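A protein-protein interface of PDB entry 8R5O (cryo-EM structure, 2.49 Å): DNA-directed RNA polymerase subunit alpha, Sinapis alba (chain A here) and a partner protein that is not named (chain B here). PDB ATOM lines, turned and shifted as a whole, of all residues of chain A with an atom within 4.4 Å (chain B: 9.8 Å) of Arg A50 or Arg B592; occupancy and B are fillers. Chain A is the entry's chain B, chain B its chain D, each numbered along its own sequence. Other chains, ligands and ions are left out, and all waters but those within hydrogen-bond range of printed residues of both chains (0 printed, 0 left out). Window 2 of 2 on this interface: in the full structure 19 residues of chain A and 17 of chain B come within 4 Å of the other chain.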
ATOM      1  N   GLY A  46      22.713 -16.296 -19.540  1.00  0.00           N
ATOM      2  CA  GLY A  46      21.424 -16.479 -20.184  1.00  0.00           C
ATOM      3  C   GLY A  46      20.281 -15.859 -19.406  1.00  0.00           C
ATOM      4  O   GLY A  46      19.360 -15.283 -19.989  1.00  0.00           O
ATOM      5  N   ILE A  47      20.319 -15.974 -18.077  1.00  0.00           N
ATOM      6  CA  ILE A  47      19.276 -15.383 -17.246  1.00  0.00           C
ATOM      7  C   ILE A  47      19.310 -13.861 -17.344  1.00  0.00           C
ATOM      8  O   ILE A  47      18.274 -13.212 -17.526  1.00  0.00           O
ATOM      9  CB  ILE A  47      19.420 -15.862 -15.791  1.00  0.00           C
ATOM     10  CG1 ILE A  47      19.096 -17.354 -15.688  1.00  0.00           C
ATOM     11  CG2 ILE A  47      18.526 -15.046 -14.872  1.00  0.00           C
ATOM     12  CD1 ILE A  47      19.703 -18.038 -14.479  1.00  0.00           C
ATOM     13  N   ALA A  48      20.501 -13.272 -17.226  1.00  0.00           N
ATOM     14  CA  ALA A  48      20.616 -11.818 -17.279  1.00  0.00           C
ATOM     15  C   ALA A  48      20.261 -11.276 -18.658  1.00  0.00           C
ATOM     16  O   ALA A  48      19.572 -10.257 -18.770  1.00  0.00           O
ATOM     17  CB  ALA A  48      22.026 -11.386 -16.883  1.00  0.00           C
ATOM     18  N   MET A  49      20.733 -11.937 -19.719  1.00  0.00           N
ATOM     19  CA  MET A  49      20.435 -11.473 -21.069  1.00  0.00           C
ATOM     20  C   MET A  49      18.942 -11.535 -21.362  1.00  0.00           C
ATOM     21  O   MET A  49      18.384 -10.609 -21.960  1.00  0.00           O
ATOM     22  CB  MET A  49      21.214 -12.295 -22.096  1.00  0.00           C
ATOM     23  CG  MET A  49      22.697 -11.979 -22.151  1.00  0.00           C
ATOM     24  SD  MET A  49      23.038 -10.315 -22.747  1.00  0.00           S
ATOM     25  CE  MET A  49      22.391 -10.411 -24.409  1.00  0.00           C
ATOM     26  N   ARG A  50      18.282 -12.618 -20.950  1.00  0.00           N
ATOM     27  CA  ARG A  50      16.855 -12.755 -21.221  1.00  0.00           C
ATOM     28  C   ARG A  50      16.053 -11.653 -20.543  1.00  0.00           C
ATOM     29  O   ARG A  50      15.163 -11.055 -21.157  1.00  0.00           O
ATOM     30  CB  ARG A  50      16.359 -14.129 -20.774  1.00  0.00           C
ATOM     31  CG  ARG A  50      14.870 -14.159 -20.510  1.00  0.00           C
ATOM     32  CD  ARG A  50      14.249 -15.505 -20.802  1.00  0.00           C
ATOM     33  NE  ARG A  50      12.796 -15.431 -20.706  1.00  0.00           N
ATOM     34  CZ  ARG A  50      11.963 -16.357 -21.156  1.00  0.00           C
ATOM     35  NH1 ARG A  50      12.405 -17.454 -21.749  1.00  0.00           N
ATOM     36  NH2 ARG A  50      10.654 -16.177 -21.010  1.00  0.00           N
ATOM     37  N   ARG A  51      16.360 -11.364 -19.278  1.00  0.00           N
ATOM     38  CA  ARG A  51      15.661 -10.291 -18.580  1.00  0.00           C
ATOM     39  C   ARG A  51      15.932  -8.941 -19.235  1.00  0.00           C
ATOM     40  O   ARG A  51      15.029  -8.107 -19.349  1.00  0.00           O
ATOM     41  CB  ARG A  51      16.061 -10.276 -17.104  1.00  0.00           C
ATOM     42  CG  ARG A  51      15.474  -9.111 -16.344  1.00  0.00           C
ATOM     43  CD  ARG A  51      15.275  -9.406 -14.870  1.00  0.00           C
ATOM     44  NE  ARG A  51      14.663  -8.259 -14.211  1.00  0.00           N
ATOM     45  CZ  ARG A  51      13.358  -8.028 -14.168  1.00  0.00           C
ATOM     46  NH1 ARG A  51      12.490  -8.879 -14.689  1.00  0.00           N
ATOM     47  NH2 ARG A  51      12.915  -6.916 -13.592  1.00  0.00           N
ATOM     48  N   ALA A  52      17.170  -8.711 -19.677  1.00  0.00           N
ATOM     49  CA  ALA A  52      17.490  -7.471 -20.376  1.00  0.00           C
ATOM     50  C   ALA A  52      16.764  -7.380 -21.713  1.00  0.00           C
ATOM     51  O   ALA A  52      16.312  -6.300 -22.107  1.00  0.00           O
ATOM     52  CB  ALA A  52      18.999  -7.356 -20.581  1.00  0.00           C
ATOM     53  N   LEU A  53      16.653  -8.501 -22.427  1.00  0.00           N
ATOM     54  CA  LEU A  53      16.014  -8.495 -23.737  1.00  0.00           C
ATOM     55  C   LEU A  53      14.520  -8.209 -23.648  1.00  0.00           C
ATOM     56  O   LEU A  53      13.952  -7.616 -24.571  1.00  0.00           O
ATOM     57  CB  LEU A  53      16.251  -9.829 -24.442  1.00  0.00           C
ATOM     58  CG  LEU A  53      17.640 -10.062 -25.037  1.00  0.00           C
ATOM     59  CD1 LEU A  53      17.875 -11.541 -25.286  1.00  0.00           C
ATOM     60  CD2 LEU A  53      17.804  -9.267 -26.320  1.00  0.00           C
ATOM     61  N   LEU A  54      13.869  -8.611 -22.560  1.00  0.00           N
ATOM     62  CA  LEU A  54      12.417  -8.541 -22.487  1.00  0.00           C
ATOM     63  C   LEU A  54      11.891  -7.240 -21.894  1.00  0.00           C
ATOM     64  O   LEU A  54      10.760  -6.853 -22.207  1.00  0.00           O
ATOM     65  CB  LEU A  54      11.873  -9.721 -21.676  1.00  0.00           C
ATOM     66  CG  LEU A  54      12.112 -11.113 -22.269  1.00  0.00           C
ATOM     67  CD1 LEU A  54      11.481 -12.189 -21.403  1.00  0.00           C
ATOM     68  CD2 LEU A  54      11.588 -11.193 -23.693  1.00  0.00           C
ATOM     69  N   GLN A 180       9.949  -9.965 -29.084  1.00  0.00           N
ATOM     70  CA  GLN A 180       8.736 -10.737 -28.844  1.00  0.00           C
ATOM     71  C   GLN A 180       8.982 -11.888 -27.879  1.00  0.00           C
ATOM     72  O   GLN A 180       8.130 -12.189 -27.037  1.00  0.00           O
ATOM     73  CB  GLN A 180       8.184 -11.267 -30.166  1.00  0.00           C
ATOM     74  CG  GLN A 180       7.911 -10.196 -31.205  1.00  0.00           C
ATOM     75  CD  GLN A 180       6.746  -9.305 -30.830  1.00  0.00           C
ATOM     76  OE1 GLN A 180       6.917  -8.281 -30.171  1.00  0.00           O
ATOM     77  NE2 GLN A 180       5.550  -9.692 -31.253  1.00  0.00           N
ATOM     78  N   ASN A 181      10.135 -12.539 -27.988  1.00  0.00           N
ATOM     79  CA  ASN A 181      10.425 -13.717 -27.187  1.00  0.00           C
ATOM     80  C   ASN A 181      11.932 -13.923 -27.164  1.00  0.00           C
ATOM     81  O   ASN A 181      12.643 -13.499 -28.077  1.00  0.00           O
ATOM     82  CB  ASN A 181       9.714 -14.953 -27.749  1.00  0.00           C
ATOM     83  CG  ASN A 181       9.735 -16.127 -26.794  1.00  0.00           C
ATOM     84  OD1 ASN A 181       9.685 -15.954 -25.578  1.00  0.00           O
ATOM     85  ND2 ASN A 181       9.812 -17.332 -27.343  1.00  0.00           N
ATOM     86  N   ALA A 182      12.409 -14.575 -26.107  1.00  0.00           N
ATOM     87  CA  ALA A 182      13.829 -14.856 -25.960  1.00  0.00           C
ATOM     88  C   ALA A 182      14.003 -16.094 -25.096  1.00  0.00           C
ATOM     89  O   ALA A 182      13.280 -16.280 -24.114  1.00  0.00           O
ATOM     90  CB  ALA A 182      14.577 -13.669 -25.347  1.00  0.00           C
ATOM     91  N   ASN A 183      14.963 -16.936 -25.467  1.00  0.00           N
ATOM     92  CA  ASN A 183      15.222 -18.165 -24.736  1.00  0.00           C
ATOM     93  C   ASN A 183      16.707 -18.481 -24.820  1.00  0.00           C
ATOM     94  O   ASN A 183      17.403 -18.042 -25.738  1.00  0.00           O
ATOM     95  CB  ASN A 183      14.384 -19.325 -25.288  1.00  0.00           C
ATOM     96  CG  ASN A 183      14.353 -20.514 -24.358  1.00  0.00           C
ATOM     97  OD1 ASN A 183      14.410 -20.364 -23.137  1.00  0.00           O
ATOM     98  ND2 ASN A 183      14.264 -21.708 -24.928  1.00  0.00           N
ATOM     99  N   PHE B 581      -6.301  -6.625 -24.914  1.00  0.00           N
ATOM    100  CA  PHE B 581      -5.120  -7.044 -25.653  1.00  0.00           C
ATOM    101  C   PHE B 581      -5.512  -7.381 -27.082  1.00  0.00           C
ATOM    102  O   PHE B 581      -6.511  -8.069 -27.312  1.00  0.00           O
ATOM    103  CB  PHE B 581      -4.440  -8.238 -24.979  1.00  0.00           C
ATOM    104  CG  PHE B 581      -3.832  -7.909 -23.648  1.00  0.00           C
ATOM    105  CD1 PHE B 581      -2.639  -7.213 -23.574  1.00  0.00           C
ATOM    106  CD2 PHE B 581      -4.454  -8.291 -22.473  1.00  0.00           C
ATOM    107  CE1 PHE B 581      -2.077  -6.905 -22.354  1.00  0.00           C
ATOM    108  CE2 PHE B 581      -3.896  -7.986 -21.251  1.00  0.00           C
ATOM    109  CZ  PHE B 581      -2.706  -7.292 -21.190  1.00  0.00           C
ATOM    110  N   SER B 584      -3.003 -12.658 -28.387  1.00  0.00           N
ATOM    111  CA  SER B 584      -2.589 -13.433 -27.222  1.00  0.00           C
ATOM    112  C   SER B 584      -1.116 -13.226 -26.896  1.00  0.00           C
ATOM    113  O   SER B 584      -0.719 -13.359 -25.733  1.00  0.00           O
ATOM    114  CB  SER B 584      -2.875 -14.916 -27.451  1.00  0.00           C
ATOM    115  OG  SER B 584      -2.038 -15.440 -28.464  1.00  0.00           O
ATOM    116  N   TYR B 585      -0.296 -12.905 -27.896  1.00  0.00           N
ATOM    117  CA  TYR B 585       1.125 -12.692 -27.644  1.00  0.00           C
ATOM    118  C   TYR B 585       1.374 -11.411 -26.858  1.00  0.00           C
ATOM    119  O   TYR B 585       2.296 -11.364 -26.036  1.00  0.00           O
ATOM    120  CB  TYR B 585       1.893 -12.679 -28.964  1.00  0.00           C
ATOM    121  CG  TYR B 585       1.649 -13.916 -29.793  1.00  0.00           C
ATOM    122  CD1 TYR B 585       2.234 -15.127 -29.455  1.00  0.00           C
ATOM    123  CD2 TYR B 585       0.822 -13.877 -30.907  1.00  0.00           C
ATOM    124  CE1 TYR B 585       2.008 -16.264 -30.205  1.00  0.00           C
ATOM    125  CE2 TYR B 585       0.590 -15.008 -31.664  1.00  0.00           C
ATOM    126  CZ  TYR B 585       1.186 -16.199 -31.308  1.00  0.00           C
ATOM    127  OH  TYR B 585       0.959 -17.330 -32.058  1.00  0.00           O
ATOM    128  N   ASP B 586       0.577 -10.367 -27.095  1.00  0.00           N
ATOM    129  CA  ASP B 586       0.691  -9.160 -26.282  1.00  0.00           C
ATOM    130  C   ASP B 586       0.296  -9.430 -24.835  1.00  0.00           C
ATOM    131  O   ASP B 586       0.925  -8.907 -23.908  1.00  0.00           O
ATOM    132  CB  ASP B 586      -0.160  -8.035 -26.867  1.00  0.00           C
ATOM    133  CG  ASP B 586       0.532  -7.310 -28.003  1.00  0.00           C
ATOM    134  OD1 ASP B 586       1.383  -7.925 -28.678  1.00  0.00           O
ATOM    135  OD2 ASP B 586       0.237  -6.115 -28.213  1.00  0.00           O
ATOM    136  N   ALA B 587      -0.748 -10.234 -24.624  1.00  0.00           N
ATOM    137  CA  ALA B 587      -1.164 -10.562 -23.264  1.00  0.00           C
ATOM    138  C   ALA B 587      -0.088 -11.352 -22.533  1.00  0.00           C
ATOM    139  O   ALA B 587       0.197 -11.091 -21.359  1.00  0.00           O
ATOM    140  CB  ALA B 587      -2.478 -11.343 -23.288  1.00  0.00           C
ATOM    141  N   ILE B 588       0.523 -12.322 -23.212  1.00  0.00           N
ATOM    142  CA  ILE B 588       1.593 -13.097 -22.597  1.00  0.00           C
ATOM    143  C   ILE B 588       2.816 -12.221 -22.360  1.00  0.00           C
ATOM    144  O   ILE B 588       3.502 -12.353 -21.340  1.00  0.00           O
ATOM    145  CB  ILE B 588       1.921 -14.326 -23.462  1.00  0.00           C
ATOM    146  CG1 ILE B 588       0.720 -15.273 -23.499  1.00  0.00           C
ATOM    147  CG2 ILE B 588       3.153 -15.043 -22.936  1.00  0.00           C
ATOM    148  CD1 ILE B 588       0.941 -16.513 -24.324  1.00  0.00           C
ATOM    149  N   GLY B 589       3.101 -11.306 -23.287  1.00  0.00           N
ATOM    150  CA  GLY B 589       4.228 -10.405 -23.102  1.00  0.00           C
ATOM    151  C   GLY B 589       4.038  -9.462 -21.930  1.00  0.00           C
ATOM    152  O   GLY B 589       4.990  -9.158 -21.207  1.00  0.00           O
ATOM    153  N   ALA B 590       2.810  -8.981 -21.729  1.00  0.00           N
ATOM    154  CA  ALA B 590       2.524  -8.155 -20.562  1.00  0.00           C
ATOM    155  C   ALA B 590       2.667  -8.945 -19.268  1.00  0.00           C
ATOM    156  O   ALA B 590       3.045  -8.381 -18.236  1.00  0.00           O
ATOM    157  CB  ALA B 590       1.121  -7.561 -20.669  1.00  0.00           C
ATOM    158  N   TYR B 591       2.368 -10.245 -19.305  1.00  0.00           N
ATOM    159  CA  TYR B 591       2.547 -11.081 -18.124  1.00  0.00           C
ATOM    160  C   TYR B 591       4.023 -11.272 -17.799  1.00  0.00           C
ATOM    161  O   TYR B 591       4.412 -11.271 -16.626  1.00  0.00           O
ATOM    162  CB  TYR B 591       1.856 -12.426 -18.335  1.00  0.00           C
ATOM    163  CG  TYR B 591       2.165 -13.459 -17.279  1.00  0.00           C
ATOM    164  CD1 TYR B 591       1.647 -13.345 -15.998  1.00  0.00           C
ATOM    165  CD2 TYR B 591       2.963 -14.556 -17.569  1.00  0.00           C
ATOM    166  CE1 TYR B 591       1.922 -14.288 -15.032  1.00  0.00           C
ATOM    167  CE2 TYR B 591       3.243 -15.505 -16.610  1.00  0.00           C
ATOM    168  CZ  TYR B 591       2.720 -15.368 -15.343  1.00  0.00           C
ATOM    169  OH  TYR B 591       2.996 -16.311 -14.381  1.00  0.00           O
ATOM    170  N   ARG B 592       4.862 -11.434 -18.826  1.00  0.00           N
ATOM    171  CA  ARG B 592       6.294 -11.587 -18.598  1.00  0.00           C
ATOM    172  C   ARG B 592       6.911 -10.324 -18.013  1.00  0.00           C
ATOM    173  O   ARG B 592       7.863 -10.404 -17.231  1.00  0.00           O
ATOM    174  CB  ARG B 592       6.995 -11.973 -19.899  1.00  0.00           C
ATOM    175  CG  ARG B 592       6.773 -13.417 -20.301  1.00  0.00           C
ATOM    176  CD  ARG B 592       7.177 -13.674 -21.741  1.00  0.00           C
ATOM    177  NE  ARG B 592       7.033 -15.083 -22.086  1.00  0.00           N
ATOM    178  CZ  ARG B 592       7.037 -15.558 -23.324  1.00  0.00           C
ATOM    179  NH1 ARG B 592       7.156 -14.759 -24.371  1.00  0.00           N
ATOM    180  NH2 ARG B 592       6.912 -16.868 -23.515  1.00  0.00           N
ATOM    181  N   GLN B 593       6.391  -9.157 -18.379  1.00  0.00           N
ATOM    182  CA  GLN B 593       6.856  -7.892 -17.833  1.00  0.00           C
ATOM    183  C   GLN B 593       6.192  -7.545 -16.507  1.00  0.00           C
ATOM    184  O   GLN B 593       6.288  -6.397 -16.062  1.00  0.00           O
ATOM    185  CB  GLN B 593       6.629  -6.767 -18.846  1.00  0.00           C
ATOM    186  CG  GLN B 593       7.516  -6.873 -20.077  1.00  0.00           C
ATOM    187  CD  GLN B 593       7.167  -5.850 -21.141  1.00  0.00           C
ATOM    188  OE1 GLN B 593       6.134  -5.189 -21.066  1.00  0.00           O
ATOM    189  NE2 GLN B 593       8.032  -5.716 -22.137  1.00  0.00           N
ATOM    190  N   LYS B 594       5.526  -8.512 -15.873  1.00  0.00           N
ATOM    191  CA  LYS B 594       4.893  -8.336 -14.566  1.00  0.00           C
ATOM    192  C   LYS B 594       3.869  -7.205 -14.570  1.00  0.00           C
ATOM    193  O   LYS B 594       3.671  -6.530 -13.558  1.00  0.00           O
ATOM    194  CB  LYS B 594       5.934  -8.106 -13.467  1.00  0.00           C
ATOM    195  CG  LYS B 594       7.005  -9.178 -13.397  1.00  0.00           C
ATOM    196  CD  LYS B 594       6.406 -10.537 -13.080  1.00  0.00           C
ATOM    197  CE  LYS B 594       7.467 -11.623 -13.070  1.00  0.00           C
ATOM    198  NZ  LYS B 594       8.110 -11.789 -14.402  1.00  0.00           N
ATOM    199  N   ARG B 595       3.207  -6.989 -15.705  1.00  0.00           N
ATOM    200  CA  ARG B 595       2.152  -5.988 -15.778  1.00  0.00           C
ATOM    201  C   ARG B 595       0.797  -6.543 -15.364  1.00  0.00           C
ATOM    202  O   ARG B 595      -0.053  -5.786 -14.883  1.00  0.00           O
ATOM    203  CB  ARG B 595       2.063  -5.414 -17.193  1.00  0.00           C
ATOM    204  CG  ARG B 595       3.402  -4.991 -17.767  1.00  0.00           C
ATOM    205  CD  ARG B 595       3.221  -4.100 -18.978  1.00  0.00           C
ATOM    206  NE  ARG B 595       2.588  -2.840 -18.614  1.00  0.00           N
ATOM    207  CZ  ARG B 595       2.218  -1.908 -19.481  1.00  0.00           C
ATOM    208  NH1 ARG B 595       2.392  -2.066 -20.781  1.00  0.00           N
ATOM    209  NH2 ARG B 595       1.658  -0.789 -19.030  1.00  0.00           N
ATOM    210  N   ILE B 596       0.577  -7.845 -15.544  1.00  0.00           N
ATOM    211  CA  ILE B 596      -0.632  -8.518 -15.098  1.00  0.00           C
ATOM    212  C   ILE B 596      -0.228  -9.799 -14.383  1.00  0.00           C
ATOM    213  O   ILE B 596       0.887 -10.303 -14.538  1.00  0.00           O
ATOM    214  CB  ILE B 596      -1.601  -8.836 -16.257  1.00  0.00           C
ATOM    215  CG1 ILE B 596      -0.906  -9.695 -17.313  1.00  0.00           C
ATOM    216  CG2 ILE B 596      -2.145  -7.558 -16.875  1.00  0.00           C
ATOM    217  CD1 ILE B 596      -1.774 -10.014 -18.497  1.00  0.00           C
ATOM    218  N   ASN B 597      -1.152 -10.325 -13.588  1.00  0.00           N
ATOM    219  CA  ASN B 597      -0.933 -11.580 -12.890  1.00  0.00           C
ATOM    220  C   ASN B 597      -1.485 -12.744 -13.709  1.00  0.00           C
ATOM    221  O   ASN B 597      -2.166 -12.564 -14.721  1.00  0.00           O
ATOM    222  CB  ASN B 597      -1.571 -11.540 -11.503  1.00  0.00           C
ATOM    223  CG  ASN B 597      -0.883 -10.558 -10.579  1.00  0.00           C
ATOM    224  OD1 ASN B 597       0.344 -10.494 -10.526  1.00  0.00           O
ATOM    225  ND2 ASN B 597      -1.672  -9.779  -9.849  1.00  0.00           N
ATOM    226  N   LEU B 598      -1.174 -13.959 -13.255  1.00  0.00           N
ATOM    227  CA  LEU B 598      -1.558 -15.153 -14.000  1.00  0.00           C
ATOM    228  C   LEU B 598      -3.070 -15.336 -14.045  1.00  0.00           C
ATOM    229  O   LEU B 598      -3.597 -15.886 -15.018  1.00  0.00           O
ATOM    230  CB  LEU B 598      -0.895 -16.387 -13.390  1.00  0.00           C
ATOM    231  CG  LEU B 598      -1.134 -17.708 -14.122  1.00  0.00           C
ATOM    232  CD1 LEU B 598      -0.461 -17.698 -15.488  1.00  0.00           C
ATOM    233  CD2 LEU B 598      -0.654 -18.879 -13.289  1.00  0.00           C
ATOM    234  N   VAL B 656      -4.373 -15.056 -18.702  1.00  0.00           N
ATOM    235  CA  VAL B 656      -3.202 -15.566 -19.404  1.00  0.00           C
ATOM    236  C   VAL B 656      -2.983 -17.044 -19.126  1.00  0.00           C
ATOM    237  O   VAL B 656      -2.356 -17.731 -19.936  1.00  0.00           O
ATOM    238  CB  VAL B 656      -1.937 -14.764 -19.051  1.00  0.00           C
ATOM    239  CG1 VAL B 656      -1.954 -13.420 -19.752  1.00  0.00           C
ATOM    240  CG2 VAL B 656      -1.822 -14.586 -17.555  1.00  0.00           C
ATOM    241  N   SER B 660      -2.252 -19.439 -21.995  1.00  0.00           N
ATOM    242  CA  SER B 660      -1.035 -20.244 -22.011  1.00  0.00           C
ATOM    243  C   SER B 660      -1.337 -21.710 -22.288  1.00  0.00           C
ATOM    244  O   SER B 660      -0.619 -22.365 -23.051  1.00  0.00           O
ATOM    245  CB  SER B 660      -0.291 -20.098 -20.683  1.00  0.00           C
ATOM    246  OG  SER B 660       0.156 -18.772 -20.489  1.00  0.00           O
ATOM    247  N   ARG B 663      -2.271 -22.068 -25.973  1.00  0.00           N
ATOM    248  CA  ARG B 663      -1.104 -21.890 -26.831  1.00  0.00           C
ATOM    249  C   ARG B 663      -0.180 -23.099 -26.781  1.00  0.00           C
ATOM    250  O   ARG B 663       0.394 -23.488 -27.804  1.00  0.00           O
ATOM    251  CB  ARG B 663      -0.351 -20.623 -26.429  1.00  0.00           C
ATOM    252  CG  ARG B 663      -0.931 -19.352 -27.018  1.00  0.00           C
ATOM    253  CD  ARG B 663      -0.375 -19.098 -28.409  1.00  0.00           C
ATOM    254  NE  ARG B 663      -1.176 -18.144 -29.166  1.00  0.00           N
ATOM    255  CZ  ARG B 663      -2.005 -18.479 -30.145  1.00  0.00           C
ATOM    256  NH1 ARG B 663      -2.164 -19.739 -30.513  1.00  0.00           N
ATOM    257  NH2 ARG B 663      -2.685 -17.526 -30.775  1.00  0.00           N
ATOM    258  N   GLU B 664      -0.015 -23.697 -25.599  1.00  0.00           N
ATOM    259  CA  GLU B 664       0.900 -24.827 -25.458  1.00  0.00           C
ATOM    260  C   GLU B 664       0.476 -25.996 -26.337  1.00  0.00           C
ATOM    261  O   GLU B 664       1.311 -26.606 -27.014  1.00  0.00           O
ATOM    262  CB  GLU B 664       0.975 -25.260 -23.994  1.00  0.00           C
ATOM    263  CG  GLU B 664       1.952 -26.392 -23.719  1.00  0.00           C
ATOM    264  CD  GLU B 664       3.388 -25.915 -23.625  1.00  0.00           C
ATOM    265  OE1 GLU B 664       3.607 -24.686 -23.598  1.00  0.00           O
ATOM    266  OE2 GLU B 664       4.297 -26.768 -23.577  1.00  0.00           O
ATOM    267  N   GLU B 667       0.713 -24.811 -30.208  1.00  0.00           N
ATOM    268  CA  GLU B 667       2.087 -24.769 -30.695  1.00  0.00           C
ATOM    269  C   GLU B 667       2.711 -26.158 -30.740  1.00  0.00           C
ATOM    270  O   GLU B 667       3.596 -26.409 -31.564  1.00  0.00           O
ATOM    271  CB  GLU B 667       2.926 -23.829 -29.830  1.00  0.00           C
ATOM    272  CG  GLU B 667       2.591 -22.363 -30.026  1.00  0.00           C
ATOM    273  CD  GLU B 667       3.373 -21.452 -29.100  1.00  0.00           C
ATOM    274  OE1 GLU B 667       4.093 -21.970 -28.222  1.00  0.00           O
ATOM    275  OE2 GLU B 667       3.266 -20.218 -29.251  1.00  0.00           O
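The side-chain amide nitrogen (NE2) of Gln B593 lies within hydrogen-bond range of the backbone carbonyl oxygen (O) of Leu A54 (3.0 Å).
The side-chain amide oxygen (OD1) of Asn A181 lies within hydrogen-bond range of the guanidinium group (NH1) of Arg B592 (3.0 Å).
O of Ala A182 sits at hydrogen-bond distance from NH1 of Arg A50 (2.8 Å).
O of Arg B592 sits at hydrogen-bond distance from NZ of Lys B594 (3.2 Å).
Among the printed residues, pairs that only touch across the chains: Gln A180 with Arg B592 and Arg A50 with Arg B592.
No residue of chain B comes within 4 Å of Ala A48.
Arg A50 touches just one residue of chain B: Arg B592 (3.9 Å).
Arg A51 touches none of the printed residues of chain B.
No residue of chain B comes within 4 Å of Ala A52.
Of the printed residues of chain B, Leu A54 touches Gln B593.
Printed residues of chain B within 4 Å of Gln A180: Arg B592.
Of the printed residues of chain B, Asn A181 touches Arg B592.
Ala A182 touches none of the printed residues of chain B.
Ile B588 touches none of the printed residues of chain A.
Of chain A, only Arg A50, Gln A180 and Asn A181 come within 4 Å of Arg B592.
Of the printed residues of chain A, Gln B593 touches Leu A54 (3.0 Å).
The nearest printed residue of chain B that does not touch Leu A54 is Arg B592 (4.6 Å).
Along chain A the printed residues that touch a printed residue of chain B span positions 50 to 181.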
